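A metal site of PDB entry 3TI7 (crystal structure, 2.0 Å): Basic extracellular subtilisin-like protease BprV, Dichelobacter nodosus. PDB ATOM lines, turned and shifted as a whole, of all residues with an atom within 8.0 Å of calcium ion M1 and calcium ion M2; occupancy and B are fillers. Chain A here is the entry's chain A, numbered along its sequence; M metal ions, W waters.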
ATOM      1  N   TYR A  58     -32.516  -8.974  -0.145  1.00  0.00           N
ATOM      2  CA  TYR A  58     -31.124  -8.600  -0.394  1.00  0.00           C
ATOM      3  C   TYR A  58     -30.927  -8.121  -1.825  1.00  0.00           C
ATOM      4  O   TYR A  58     -31.601  -8.579  -2.748  1.00  0.00           O
ATOM      5  CB  TYR A  58     -30.161  -9.768  -0.083  1.00  0.00           C
ATOM      6  CG  TYR A  58     -28.762  -9.295   0.209  1.00  0.00           C
ATOM      7  CD1 TYR A  58     -28.371  -8.941   1.511  1.00  0.00           C
ATOM      8  CD2 TYR A  58     -27.809  -9.193  -0.810  1.00  0.00           C
ATOM      9  CE1 TYR A  58     -27.078  -8.486   1.777  1.00  0.00           C
ATOM     10  CE2 TYR A  58     -26.524  -8.743  -0.554  1.00  0.00           C
ATOM     11  CZ  TYR A  58     -26.160  -8.385   0.729  1.00  0.00           C
ATOM     12  OH  TYR A  58     -24.886  -7.948   0.970  1.00  0.00           O
ATOM     13  N   ASP A  59     -29.991  -7.191  -2.003  1.00  0.00           N
ATOM     14  CA  ASP A  59     -29.684  -6.633  -3.317  1.00  0.00           C
ATOM     15  C   ASP A  59     -28.378  -7.240  -3.832  1.00  0.00           C
ATOM     16  O   ASP A  59     -27.288  -6.923  -3.346  1.00  0.00           O
ATOM     17  CB  ASP A  59     -29.569  -5.108  -3.206  1.00  0.00           C
ATOM     18  CG  ASP A  59     -29.486  -4.389  -4.553  1.00  0.00           C
ATOM     19  OD1 ASP A  59     -28.989  -4.969  -5.541  1.00  0.00           O
ATOM     20  OD2 ASP A  59     -29.902  -3.210  -4.615  1.00  0.00           O
ATOM     21  N   PHE A  60     -28.511  -8.116  -4.838  1.00  0.00           N
ATOM     22  CA  PHE A  60     -27.360  -8.831  -5.397  1.00  0.00           C
ATOM     23  C   PHE A  60     -26.713  -8.175  -6.624  1.00  0.00           C
ATOM     24  O   PHE A  60     -25.758  -8.729  -7.181  1.00  0.00           O
ATOM     25  CB  PHE A  60     -27.730 -10.293  -5.719  1.00  0.00           C
ATOM     26  CG  PHE A  60     -27.792 -11.175  -4.504  1.00  0.00           C
ATOM     27  CD1 PHE A  60     -26.654 -11.888  -4.080  1.00  0.00           C
ATOM     28  CD2 PHE A  60     -28.963 -11.278  -3.752  1.00  0.00           C
ATOM     29  CE1 PHE A  60     -26.689 -12.692  -2.938  1.00  0.00           C
ATOM     30  CE2 PHE A  60     -29.014 -12.086  -2.614  1.00  0.00           C
ATOM     31  CZ  PHE A  60     -27.874 -12.795  -2.204  1.00  0.00           C
ATOM     32  N   ILE A  61     -27.210  -6.999  -7.036  1.00  0.00           N
ATOM     33  CA  ILE A  61     -26.642  -6.329  -8.218  1.00  0.00           C
ATOM     34  C   ILE A  61     -25.227  -5.851  -7.923  1.00  0.00           C
ATOM     35  O   ILE A  61     -25.016  -4.973  -7.078  1.00  0.00           O
ATOM     36  CB  ILE A  61     -27.527  -5.145  -8.755  1.00  0.00           C
ATOM     37  CG1 ILE A  61     -28.964  -5.593  -9.028  1.00  0.00           C
ATOM     38  CG2 ILE A  61     -26.891  -4.542 -10.034  1.00  0.00           C
ATOM     39  CD1 ILE A  61     -29.926  -4.435  -9.289  1.00  0.00           C
ATOM     40  N   SER A  62     -24.266  -6.438  -8.620  1.00  0.00           N
ATOM     41  CA  SER A  62     -22.844  -6.142  -8.427  1.00  0.00           C
ATOM     42  C   SER A  62     -22.406  -4.820  -9.059  1.00  0.00           C
ATOM     43  O   SER A  62     -21.469  -4.169  -8.584  1.00  0.00           O
ATOM     44  CB  SER A  62     -21.983  -7.292  -8.935  1.00  0.00           C
ATOM     45  OG  SER A  62     -22.235  -8.483  -8.201  1.00  0.00           O
ATOM     46  N   SER A  63     -23.081  -4.415 -10.133  1.00  0.00           N
ATOM     47  CA  SER A  63     -22.821  -3.122 -10.768  1.00  0.00           C
ATOM     48  C   SER A  63     -23.502  -1.959 -10.026  1.00  0.00           C
ATOM     49  O   SER A  63     -24.730  -1.847 -10.036  1.00  0.00           O
ATOM     50  CB  SER A  63     -23.279  -3.159 -12.232  1.00  0.00           C
ATOM     51  OG  SER A  63     -23.202  -1.879 -12.827  1.00  0.00           O
ATOM     52  N   ALA A  64     -22.696  -1.111  -9.380  1.00  0.00           N
ATOM     53  CA  ALA A  64     -23.204   0.096  -8.722  1.00  0.00           C
ATOM     54  C   ALA A  64     -23.967   1.041  -9.675  1.00  0.00           C
ATOM     55  O   ALA A  64     -25.037   1.539  -9.288  1.00  0.00           O
ATOM     56  CB  ALA A  64     -22.104   0.840  -7.979  1.00  0.00           C
ATOM     57  N   PRO A  65     -23.422   1.295 -10.884  1.00  0.00           N
ATOM     58  CA  PRO A  65     -24.141   2.068 -11.907  1.00  0.00           C
ATOM     59  C   PRO A  65     -25.555   1.541 -12.221  1.00  0.00           C
ATOM     60  O   PRO A  65     -26.524   2.300 -12.209  1.00  0.00           O
ATOM     61  CB  PRO A  65     -23.251   1.929 -13.139  1.00  0.00           C
ATOM     62  CG  PRO A  65     -21.883   1.814 -12.587  1.00  0.00           C
ATOM     63  CD  PRO A  65     -22.074   0.945 -11.374  1.00  0.00           C
ATOM     64  N   ASN A  66     -25.650   0.248 -12.503  1.00  0.00           N
ATOM     65  CA  ASN A  66     -26.914  -0.343 -12.890  1.00  0.00           C
ATOM     66  C   ASN A  66     -27.903  -0.507 -11.725  1.00  0.00           C
ATOM     67  O   ASN A  66     -29.103  -0.551 -11.940  1.00  0.00           O
ATOM     68  CB  ASN A  66     -26.679  -1.668 -13.630  1.00  0.00           C
ATOM     69  CG  ASN A  66     -25.959  -1.477 -14.962  1.00  0.00           C
ATOM     70  OD1 ASN A  66     -25.863  -0.372 -15.495  1.00  0.00           O
ATOM     71  ND2 ASN A  66     -25.457  -2.579 -15.521  1.00  0.00           N
ATOM     72  N   ALA A  67     -27.384  -0.545 -10.498  1.00  0.00           N
ATOM     73  CA  ALA A  67     -28.219  -0.631  -9.293  1.00  0.00           C
ATOM     74  C   ALA A  67     -28.812   0.723  -8.832  1.00  0.00           C
ATOM     75  O   ALA A  67     -29.791   0.754  -8.067  1.00  0.00           O
ATOM     76  CB  ALA A  67     -27.453  -1.292  -8.167  1.00  0.00           C
ATOM     77  N   ARG A  68     -28.195   1.814  -9.281  1.00  0.00           N
ATOM     78  CA  ARG A  68     -28.620   3.197  -8.995  1.00  0.00           C
ATOM     79  C   ARG A  68     -28.762   3.561  -7.514  1.00  0.00           C
ATOM     80  O   ARG A  68     -29.574   4.410  -7.146  1.00  0.00           O
ATOM     81  CB  ARG A  68     -29.903   3.556  -9.763  1.00  0.00           C
ATOM     82  CG  ARG A  68     -29.667   3.876 -11.237  1.00  0.00           C
ATOM     83  CD  ARG A  68     -30.977   3.939 -11.996  1.00  0.00           C
ATOM     84  NE  ARG A  68     -30.819   4.540 -13.321  1.00  0.00           N
ATOM     85  CZ  ARG A  68     -31.486   4.171 -14.409  1.00  0.00           C
ATOM     86  NH1 ARG A  68     -32.370   3.164 -14.349  1.00  0.00           N
ATOM     87  NH2 ARG A  68     -31.267   4.794 -15.554  1.00  0.00           N
ATOM     88  N   ASP A  69     -27.955   2.924  -6.662  1.00  0.00           N
ATOM     89  CA  ASP A  69     -28.084   3.146  -5.223  1.00  0.00           C
ATOM     90  C   ASP A  69     -26.764   3.510  -4.536  1.00  0.00           C
ATOM     91  O   ASP A  69     -26.696   3.570  -3.313  1.00  0.00           O
ATOM     92  CB  ASP A  69     -28.720   1.908  -4.564  1.00  0.00           C
ATOM     93  CG  ASP A  69     -27.939   0.635  -4.856  1.00  0.00           C
ATOM     94  OD1 ASP A  69     -26.791   0.719  -5.330  1.00  0.00           O
ATOM     95  OD2 ASP A  69     -28.478  -0.458  -4.586  1.00  0.00           O
ATOM     96  N   GLY A  70     -25.722   3.743  -5.331  1.00  0.00           N
ATOM     97  CA  GLY A  70     -24.425   4.189  -4.831  1.00  0.00           C
ATOM     98  C   GLY A  70     -23.399   3.131  -4.446  1.00  0.00           C
ATOM     99  O   GLY A  70     -22.253   3.475  -4.115  1.00  0.00           O
ATOM    100  N   ASP A  71     -23.775   1.862  -4.501  1.00  0.00           N
ATOM    101  CA  ASP A  71     -22.876   0.775  -4.102  1.00  0.00           C
ATOM    102  C   ASP A  71     -23.095  -0.547  -4.859  1.00  0.00           C
ATOM    103  O   ASP A  71     -23.990  -0.649  -5.698  1.00  0.00           O
ATOM    104  CB  ASP A  71     -22.935   0.538  -2.590  1.00  0.00           C
ATOM    105  CG  ASP A  71     -24.344   0.272  -2.075  1.00  0.00           C
ATOM    106  OD1 ASP A  71     -25.210  -0.201  -2.839  1.00  0.00           O
ATOM    107  OD2 ASP A  71     -24.594   0.551  -0.888  1.00  0.00           O
ATOM    108  N   GLN A  72     -22.292  -1.551  -4.545  1.00  0.00           N
ATOM    109  CA  GLN A  72     -22.453  -2.865  -5.144  1.00  0.00           C
ATOM    110  C   GLN A  72     -23.475  -3.666  -4.331  1.00  0.00           C
ATOM    111  O   GLN A  72     -24.529  -3.121  -3.986  1.00  0.00           O
ATOM    112  CB  GLN A  72     -21.099  -3.556  -5.323  1.00  0.00           C
ATOM    113  CG  GLN A  72     -20.155  -2.766  -6.222  1.00  0.00           C
ATOM    114  CD  GLN A  72     -18.867  -3.515  -6.541  1.00  0.00           C
ATOM    115  OE1 GLN A  72     -17.957  -3.592  -5.711  1.00  0.00           O
ATOM    116  NE2 GLN A  72     -18.780  -4.056  -7.745  1.00  0.00           N
ATOM    117  N   ARG A  73     -23.211  -4.926  -3.998  1.00  0.00           N
ATOM    118  CA  ARG A  73     -24.190  -5.685  -3.208  1.00  0.00           C
ATOM    119  C   ARG A  73     -24.447  -5.055  -1.841  1.00  0.00           C
ATOM    120  O   ARG A  73     -23.532  -4.520  -1.206  1.00  0.00           O
ATOM    121  CB  ARG A  73     -23.819  -7.165  -3.112  1.00  0.00           C
ATOM    122  CG  ARG A  73     -23.795  -7.854  -4.458  1.00  0.00           C
ATOM    123  CD  ARG A  73     -23.526  -9.349  -4.316  1.00  0.00           C
ATOM    124  NE  ARG A  73     -23.732 -10.072  -5.568  1.00  0.00           N
ATOM    125  CZ  ARG A  73     -23.488 -11.366  -5.739  1.00  0.00           C
ATOM    126  NH1 ARG A  73     -23.009 -12.105  -4.729  1.00  0.00           N
ATOM    127  NH2 ARG A  73     -23.706 -11.939  -6.916  1.00  0.00           N
ATOM    128  N   ASP A  74     -25.699  -5.098  -1.401  1.00  0.00           N
ATOM    129  CA  ASP A  74     -26.137  -4.416  -0.183  1.00  0.00           C
ATOM    130  C   ASP A  74     -27.440  -5.032   0.329  1.00  0.00           C
ATOM    131  O   ASP A  74     -28.080  -5.809  -0.377  1.00  0.00           O
ATOM    132  CB  ASP A  74     -26.306  -2.911  -0.440  1.00  0.00           C
ATOM    133  CG  ASP A  74     -27.439  -2.613  -1.396  1.00  0.00           C
ATOM    134  OD1 ASP A  74     -27.247  -2.693  -2.627  1.00  0.00           O
ATOM    135  OD2 ASP A  74     -28.543  -2.288  -0.918  1.00  0.00           O
ATOM    136  N   ASN A  75     -27.835  -4.661   1.548  1.00  0.00           N
ATOM    137  CA  ASN A  75     -28.996  -5.286   2.211  1.00  0.00           C
ATOM    138  C   ASN A  75     -30.345  -4.624   1.968  1.00  0.00           C
ATOM    139  O   ASN A  75     -31.329  -4.938   2.653  1.00  0.00           O
ATOM    140  CB  ASN A  75     -28.731  -5.451   3.721  1.00  0.00           C
ATOM    141  CG  ASN A  75     -28.574  -4.121   4.446  1.00  0.00           C
ATOM    142  OD1 ASN A  75     -28.775  -3.055   3.870  1.00  0.00           O
ATOM    143  ND2 ASN A  75     -28.224  -4.194   5.730  1.00  0.00           N
ATOM    144  N   ASN A  76     -30.400  -3.711   0.996  1.00  0.00           N
ATOM    145  CA  ASN A  76     -31.637  -3.012   0.672  1.00  0.00           C
ATOM    146  C   ASN A  76     -32.055  -3.289  -0.774  1.00  0.00           C
ATOM    147  O   ASN A  76     -31.527  -2.665  -1.683  1.00  0.00           O
ATOM    148  CB  ASN A  76     -31.467  -1.495   0.904  1.00  0.00           C
ATOM    149  CG  ASN A  76     -32.745  -0.696   0.632  1.00  0.00           C
ATOM    150  OD1 ASN A  76     -33.730  -1.236   0.136  1.00  0.00           O
ATOM    151  ND2 ASN A  76     -32.731   0.588   0.989  1.00  0.00           N
ATOM    152  N   PRO A  77     -33.007  -4.236  -0.979  1.00  0.00           N
ATOM    153  CA  PRO A  77     -33.437  -4.564  -2.347  1.00  0.00           C
ATOM    154  C   PRO A  77     -34.453  -3.573  -2.953  1.00  0.00           C
ATOM    155  O   PRO A  77     -35.260  -3.980  -3.781  1.00  0.00           O
ATOM    156  CB  PRO A  77     -34.056  -5.959  -2.184  1.00  0.00           C
ATOM    157  CG  PRO A  77     -34.703  -5.893  -0.823  1.00  0.00           C
ATOM    158  CD  PRO A  77     -33.717  -5.062   0.024  1.00  0.00           C
ATOM    159  N   ALA A  78     -34.413  -2.311  -2.531  1.00  0.00           N
ATOM    160  CA  ALA A  78     -35.284  -1.270  -3.109  1.00  0.00           C
ATOM    161  C   ALA A  78     -35.106  -1.184  -4.626  1.00  0.00           C
ATOM    162  O   ALA A  78     -33.990  -1.190  -5.130  1.00  0.00           O
ATOM    163  CB  ALA A  78     -35.002   0.093  -2.464  1.00  0.00           C
ATOM    164  N   ASP A  79     -36.227  -1.150  -5.355  1.00  0.00           N
ATOM    165  CA  ASP A  79     -36.180  -0.990  -6.806  1.00  0.00           C
ATOM    166  C   ASP A  79     -36.008   0.490  -7.083  1.00  0.00           C
ATOM    167  O   ASP A  79     -36.938   1.279  -6.871  1.00  0.00           O
ATOM    168  CB  ASP A  79     -37.446  -1.526  -7.486  1.00  0.00           C
ATOM    169  CG  ASP A  79     -37.340  -1.569  -9.024  1.00  0.00           C
ATOM    170  OD1 ASP A  79     -36.337  -1.059  -9.603  1.00  0.00           O
ATOM    171  OD2 ASP A  79     -38.252  -2.122  -9.672  1.00  0.00           O
ATOM    172  N   GLU A  80     -34.814   0.867  -7.540  1.00  0.00           N
ATOM    173  CA  GLU A  80     -34.503   2.269  -7.822  1.00  0.00           C
ATOM    174  C   GLU A  80     -35.075   2.736  -9.168  1.00  0.00           C
ATOM    175  O   GLU A  80     -35.088   3.926  -9.460  1.00  0.00           O
ATOM    176  CB  GLU A  80     -32.990   2.517  -7.761  1.00  0.00           C
ATOM    177  CG  GLU A  80     -32.298   1.936  -6.512  1.00  0.00           C
ATOM    178  CD  GLU A  80     -32.511   2.744  -5.255  1.00  0.00           C
ATOM    179  OE1 GLU A  80     -33.030   3.887  -5.354  1.00  0.00           O
ATOM    180  OE2 GLU A  80     -32.153   2.245  -4.155  1.00  0.00           O
ATOM    181  N   ARG A 136     -33.148  -8.720  -5.139  1.00  0.00           N
ATOM    182  CA  ARG A 136     -32.901  -7.813  -6.261  1.00  0.00           C
ATOM    183  C   ARG A 136     -31.667  -8.222  -7.052  1.00  0.00           C
ATOM    184  O   ARG A 136     -30.553  -8.245  -6.510  1.00  0.00           O
ATOM    185  CB  ARG A 136     -32.801  -6.362  -5.798  1.00  0.00           C
ATOM    186  CG  ARG A 136     -32.782  -5.388  -6.964  1.00  0.00           C
ATOM    187  CD  ARG A 136     -32.512  -3.987  -6.514  1.00  0.00           C
ATOM    188  NE  ARG A 136     -32.730  -3.021  -7.594  1.00  0.00           N
ATOM    189  CZ  ARG A 136     -32.005  -1.926  -7.771  1.00  0.00           C
ATOM    190  NH1 ARG A 136     -30.979  -1.657  -6.963  1.00  0.00           N
ATOM    191  NH2 ARG A 136     -32.282  -1.098  -8.775  1.00  0.00           N
HETATM  192 CA    CA M   1     -26.137  -1.555  -4.400  1.00  0.00          CA
HETATM  193 CA    CA M   2     -29.818  -1.538  -2.862  1.00  0.00          CA
HETATM  194  O   HOH W   1     -31.543  -0.481  -3.939  1.00  0.00           O
HETATM  195  O   HOH W   2     -26.516  -3.108  -5.741  1.00  0.00           O
HETATM  196  O   HOH W   3     -29.580   0.237  -1.540  1.00  0.00           O
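Water W2 lies within hydrogen-bond range of the backbone carbonyl oxygen (O) of Ile 61 (2.7 Å) and the side-chain carboxylate (OD1) of Asp 59 (3.1 Å).
Water W1 lies within hydrogen-bond range of OE2 of Glu 80, O of Ala 78 and NH1 of Arg 136.
Four residues have an atom within 4 Å of calcium ion M2: Asp 59, Asp 69, Asp 74 and Asn 76.
Calcium ion M2 is bound by water W3 (2.2 Å), water W1 (2.3 Å), O of Asn 76 (2.4 Å), OD2 of Asp 59 (2.4 Å), OD2 of Asp 69 (2.4 Å), OD2 of Asp 74 (2.4 Å) and OD1 of Asp 74 (2.8 Å).
Calcium ion M2 has seven donor atoms within binding distance.
Merely in contact with calcium ion M1: Ala 67 (3.999 Å).
Of the 24 residues printed, 5 come within 4 Å of calcium ion M1.
Along chain A the residues within 4 Å of calcium ion M1 span positions 67 to 74.
Water W2 binds calcium ion M1 (2.1 Å).
Calcium ion M1 is bound by the side-chain carboxylate (OD1) of Asp 71 (2.3 Å).
The backbone carbonyl oxygen (O) of Gln 72 binds calcium ion M1 (2.3 Å).
OD1 of Asp 74 is bound to calcium ion M1, at 2.4 Å.
OD1 of Asp 69 binds calcium ion M1, at 2.5 Å.
Calcium ion M1 is bound by the side-chain carboxylate (OD2) of Asp 69 (2.6 Å).
The backbone carbonyl oxygen (O) of Asp 71 is bound to calcium ion M1 (2.7 Å).
NE2 of Gln 72 is in hydrogen-bond range of O of Ser 62 (2.8 Å).
The side-chain amide oxygen of Asn 76 sits at hydrogen-bond distance from the backbone NH of Ala 78 (3.0 Å).
The side-chain carboxylate (OD2) of Asp 59 lies close to the guanidinium group (NH1) of Arg 136.
The side-chain carboxylate of Asp 59 sits at hydrogen-bond distance from the backbone NH of Ile 61 (3.1 Å).
The side-chain carboxylate (OD2) of Asp 69 sits close to the guanidinium group (NH1) of Arg 136, 3.7 Å away.
The backbone carbonyl oxygen (O) of Ala 67 is in hydrogen-bond range of the guanidinium group (NH1) of Arg 136, 2.9 Å away.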
